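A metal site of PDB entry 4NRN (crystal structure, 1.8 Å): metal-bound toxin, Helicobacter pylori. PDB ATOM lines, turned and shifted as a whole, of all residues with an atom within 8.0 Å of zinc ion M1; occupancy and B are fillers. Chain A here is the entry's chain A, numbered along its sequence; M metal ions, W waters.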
ATOM      1  N   LYS A  45      21.115  10.631 -32.544  1.00  0.00           N
ATOM      2  CA  LYS A  45      20.519  11.808 -31.940  1.00  0.00           C
ATOM      3  C   LYS A  45      21.502  12.987 -31.969  1.00  0.00           C
ATOM      4  O   LYS A  45      22.692  12.843 -31.637  1.00  0.00           O
ATOM      5  CB  LYS A  45      20.017  11.496 -30.536  1.00  0.00           C
ATOM      6  CG  LYS A  45      18.764  10.616 -30.530  1.00  0.00           C
ATOM      7  CD  LYS A  45      18.437  10.040 -29.159  1.00  0.00           C
ATOM      8  CE  LYS A  45      17.254   9.078 -29.221  1.00  0.00           C
ATOM      9  NZ  LYS A  45      17.007   8.357 -27.929  1.00  0.00           N
ATOM     10  N   ASP A  46      20.993  14.135 -32.396  1.00  0.00           N
ATOM     11  CA  ASP A  46      21.831  15.303 -32.684  1.00  0.00           C
ATOM     12  C   ASP A  46      21.144  16.567 -32.211  1.00  0.00           C
ATOM     13  O   ASP A  46      20.047  16.899 -32.665  1.00  0.00           O
ATOM     14  CB  ASP A  46      22.080  15.400 -34.183  1.00  0.00           C
ATOM     15  CG  ASP A  46      23.036  16.504 -34.540  1.00  0.00           C
ATOM     16  OD1 ASP A  46      24.235  16.366 -34.220  1.00  0.00           O
ATOM     17  OD2 ASP A  46      22.597  17.507 -35.140  1.00  0.00           O
ATOM     18  N   HIS A  47      21.790  17.291 -31.303  1.00  0.00           N
ATOM     19  CA  HIS A  47      21.214  18.524 -30.821  1.00  0.00           C
ATOM     20  C   HIS A  47      22.337  19.445 -30.379  1.00  0.00           C
ATOM     21  O   HIS A  47      23.463  19.011 -30.182  1.00  0.00           O
ATOM     22  CB  HIS A  47      20.255  18.255 -29.665  1.00  0.00           C
ATOM     23  CG  HIS A  47      20.893  17.525 -28.533  1.00  0.00           C
ATOM     24  ND1 HIS A  47      21.596  18.162 -27.536  1.00  0.00           N
ATOM     25  CD2 HIS A  47      20.991  16.202 -28.266  1.00  0.00           C
ATOM     26  CE1 HIS A  47      22.069  17.271 -26.688  1.00  0.00           C
ATOM     27  NE2 HIS A  47      21.720  16.067 -27.110  1.00  0.00           N
ATOM     28  N   PRO A  48      22.033  20.740 -30.224  1.00  0.00           N
ATOM     29  CA  PRO A  48      23.031  21.657 -29.675  1.00  0.00           C
ATOM     30  C   PRO A  48      23.403  21.282 -28.246  1.00  0.00           C
ATOM     31  O   PRO A  48      22.598  20.654 -27.536  1.00  0.00           O
ATOM     32  CB  PRO A  48      22.305  23.004 -29.679  1.00  0.00           C
ATOM     33  CG  PRO A  48      21.306  22.885 -30.771  1.00  0.00           C
ATOM     34  CD  PRO A  48      20.854  21.451 -30.741  1.00  0.00           C
ATOM     35  N   LEU A  49      24.611  21.643 -27.835  1.00  0.00           N
ATOM     36  CA  LEU A  49      25.010  21.511 -26.446  1.00  0.00           C
ATOM     37  C   LEU A  49      24.445  22.677 -25.638  1.00  0.00           C
ATOM     38  O   LEU A  49      24.907  23.813 -25.796  1.00  0.00           O
ATOM     39  CB  LEU A  49      26.527  21.492 -26.321  1.00  0.00           C
ATOM     40  CG  LEU A  49      27.187  20.120 -26.247  1.00  0.00           C
ATOM     41  CD1 LEU A  49      28.664  20.273 -25.941  1.00  0.00           C
ATOM     42  CD2 LEU A  49      26.499  19.281 -25.188  1.00  0.00           C
ATOM     43  N   ARG A  57      27.592  21.235 -30.824  1.00  0.00           N
ATOM     44  CA  ARG A  57      26.525  20.257 -30.962  1.00  0.00           C
ATOM     45  C   ARG A  57      26.971  18.897 -30.452  1.00  0.00           C
ATOM     46  O   ARG A  57      28.162  18.655 -30.235  1.00  0.00           O
ATOM     47  CB  ARG A  57      26.024  20.140 -32.408  1.00  0.00           C
ATOM     48  CG  ARG A  57      25.412  21.415 -32.961  1.00  0.00           C
ATOM     49  CD  ARG A  57      24.764  21.168 -34.305  1.00  0.00           C
ATOM     50  NE  ARG A  57      23.550  20.373 -34.190  1.00  0.00           N
ATOM     51  CZ  ARG A  57      22.331  20.885 -34.083  1.00  0.00           C
ATOM     52  NH1 ARG A  57      22.147  22.201 -34.061  1.00  0.00           N
ATOM     53  NH2 ARG A  57      21.278  20.079 -33.982  1.00  0.00           N
ATOM     54  N   GLU A  58      25.993  18.016 -30.266  1.00  0.00           N
ATOM     55  CA  GLU A  58      26.215  16.742 -29.624  1.00  0.00           C
ATOM     56  C   GLU A  58      25.528  15.663 -30.443  1.00  0.00           C
ATOM     57  O   GLU A  58      24.316  15.695 -30.646  1.00  0.00           O
ATOM     58  CB  GLU A  58      25.627  16.794 -28.221  1.00  0.00           C
ATOM     59  CG  GLU A  58      26.153  15.749 -27.269  1.00  0.00           C
ATOM     60  CD  GLU A  58      25.552  15.915 -25.896  1.00  0.00           C
ATOM     61  OE1 GLU A  58      26.276  16.360 -24.970  1.00  0.00           O
ATOM     62  OE2 GLU A  58      24.351  15.622 -25.734  1.00  0.00           O
ATOM     63  N   CYS A  59      26.322  14.709 -30.921  1.00  0.00           N
ATOM     64  CA  CYS A  59      25.795  13.603 -31.714  1.00  0.00           C
ATOM     65  C   CYS A  59      25.956  12.310 -30.948  1.00  0.00           C
ATOM     66  O   CYS A  59      27.009  12.041 -30.375  1.00  0.00           O
ATOM     67  CB  CYS A  59      26.520  13.500 -33.058  1.00  0.00           C
ATOM     68  SG  CYS A  59      25.690  12.351 -34.142  1.00  0.00           S
ATOM     69  N   HIS A  60      24.902  11.510 -30.932  1.00  0.00           N
ATOM     70  CA  HIS A  60      24.925  10.222 -30.248  1.00  0.00           C
ATOM     71  C   HIS A  60      25.359   9.110 -31.205  1.00  0.00           C
ATOM     72  O   HIS A  60      24.542   8.591 -31.956  1.00  0.00           O
ATOM     73  CB  HIS A  60      23.547   9.941 -29.652  1.00  0.00           C
ATOM     74  CG  HIS A  60      23.244  10.783 -28.454  1.00  0.00           C
ATOM     75  ND1 HIS A  60      23.149  10.264 -27.179  1.00  0.00           N
ATOM     76  CD2 HIS A  60      23.021  12.115 -28.327  1.00  0.00           C
ATOM     77  CE1 HIS A  60      22.872  11.234 -26.326  1.00  0.00           C
ATOM     78  NE2 HIS A  60      22.793  12.368 -27.001  1.00  0.00           N
ATOM     79  N   LYS A  62      26.535   6.334 -30.122  1.00  0.00           N
ATOM     80  CA  LYS A  62      25.815   5.306 -29.398  1.00  0.00           C
ATOM     81  C   LYS A  62      25.124   6.081 -28.284  1.00  0.00           C
ATOM     82  O   LYS A  62      25.577   7.158 -27.911  1.00  0.00           O
ATOM     83  CB  LYS A  62      26.794   4.269 -28.849  1.00  0.00           C
ATOM     84  CG  LYS A  62      27.611   3.544 -29.915  1.00  0.00           C
ATOM     85  CD  LYS A  62      28.598   2.555 -29.301  1.00  0.00           C
ATOM     86  CE  LYS A  62      29.643   2.098 -30.305  1.00  0.00           C
ATOM     87  NZ  LYS A  62      30.726   1.262 -29.692  1.00  0.00           N
ATOM     88  N   PRO A  63      24.006   5.547 -27.759  1.00  0.00           N
ATOM     89  CA  PRO A  63      23.254   6.345 -26.770  1.00  0.00           C
ATOM     90  C   PRO A  63      24.115   6.962 -25.658  1.00  0.00           C
ATOM     91  O   PRO A  63      23.712   7.994 -25.105  1.00  0.00           O
ATOM     92  CB  PRO A  63      22.237   5.343 -26.223  1.00  0.00           C
ATOM     93  CG  PRO A  63      22.018   4.398 -27.381  1.00  0.00           C
ATOM     94  CD  PRO A  63      23.356   4.254 -28.038  1.00  0.00           C
ATOM     95  N   LEU A  66      29.291  10.002 -27.237  1.00  0.00           N
ATOM     96  CA  LEU A  66      28.981  11.310 -27.817  1.00  0.00           C
ATOM     97  C   LEU A  66      30.117  11.882 -28.677  1.00  0.00           C
ATOM     98  O   LEU A  66      31.295  11.800 -28.313  1.00  0.00           O
ATOM     99  CB  LEU A  66      28.643  12.295 -26.700  1.00  0.00           C
ATOM    100  CG  LEU A  66      27.722  11.707 -25.612  1.00  0.00           C
ATOM    101  CD1 LEU A  66      27.513  12.684 -24.452  1.00  0.00           C
ATOM    102  CD2 LEU A  66      26.381  11.266 -26.229  1.00  0.00           C
ATOM    103  N   HIS A  86      29.069  10.663 -21.445  1.00  0.00           N
ATOM    104  CA  HIS A  86      28.674  11.837 -20.681  1.00  0.00           C
ATOM    105  C   HIS A  86      29.620  11.991 -19.485  1.00  0.00           C
ATOM    106  O   HIS A  86      30.162  13.071 -19.239  1.00  0.00           O
ATOM    107  CB  HIS A  86      27.244  11.711 -20.188  1.00  0.00           C
ATOM    108  CG  HIS A  86      26.218  11.909 -21.259  1.00  0.00           C
ATOM    109  ND1 HIS A  86      25.595  10.860 -21.906  1.00  0.00           N
ATOM    110  CD2 HIS A  86      25.694  13.038 -21.795  1.00  0.00           C
ATOM    111  CE1 HIS A  86      24.743  11.326 -22.798  1.00  0.00           C
ATOM    112  NE2 HIS A  86      24.785  12.647 -22.752  1.00  0.00           N
ATOM    113  N   PHE A  90      31.891  15.431 -19.304  1.00  0.00           N
ATOM    114  CA  PHE A  90      31.262  16.433 -18.443  1.00  0.00           C
ATOM    115  C   PHE A  90      31.581  16.212 -16.964  1.00  0.00           C
ATOM    116  O   PHE A  90      31.720  15.084 -16.504  1.00  0.00           O
ATOM    117  CB  PHE A  90      29.747  16.436 -18.671  1.00  0.00           C
ATOM    118  CG  PHE A  90      29.339  16.554 -20.115  1.00  0.00           C
ATOM    119  CD1 PHE A  90      29.759  17.633 -20.876  1.00  0.00           C
ATOM    120  CD2 PHE A  90      28.550  15.588 -20.715  1.00  0.00           C
ATOM    121  CE1 PHE A  90      29.404  17.747 -22.208  1.00  0.00           C
ATOM    122  CE2 PHE A  90      28.186  15.696 -22.057  1.00  0.00           C
ATOM    123  CZ  PHE A  90      28.610  16.783 -22.795  1.00  0.00           C
HETATM  124 ZN    ZN M   1      22.508  14.161 -26.201  1.00  0.00          ZN
HETATM  125 ZN    ZN M   2      23.295  14.579 -23.449  1.00  0.00          ZN
HETATM  126  O   HOH W   1      20.043  13.271 -26.147  1.00  0.00           O
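The backbone NH (N) of His 60 sits at hydrogen-bond distance from the backbone carbonyl oxygen (O) of Lys 45 (2.7 Å).
ND1 of His 60 sits at hydrogen-bond distance from O of Pro 63, at 3.1 Å.
Within 4 Å of zinc ion M1: His 47, Glu 58 and His 60.
The nearest printed residue that does not touch zinc ion M1 is His 86 (4.4 Å).
Zinc ion M1 is bound by a ring nitrogen (NE2) of His 60 (2.0 Å), a ring nitrogen (NE2) of His 47 (2.3 Å) and the side-chain carboxylate of Glu 58 (2.4 Å).
Slightly farther from zinc ion M1 lies water W1 (2.6 Å).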
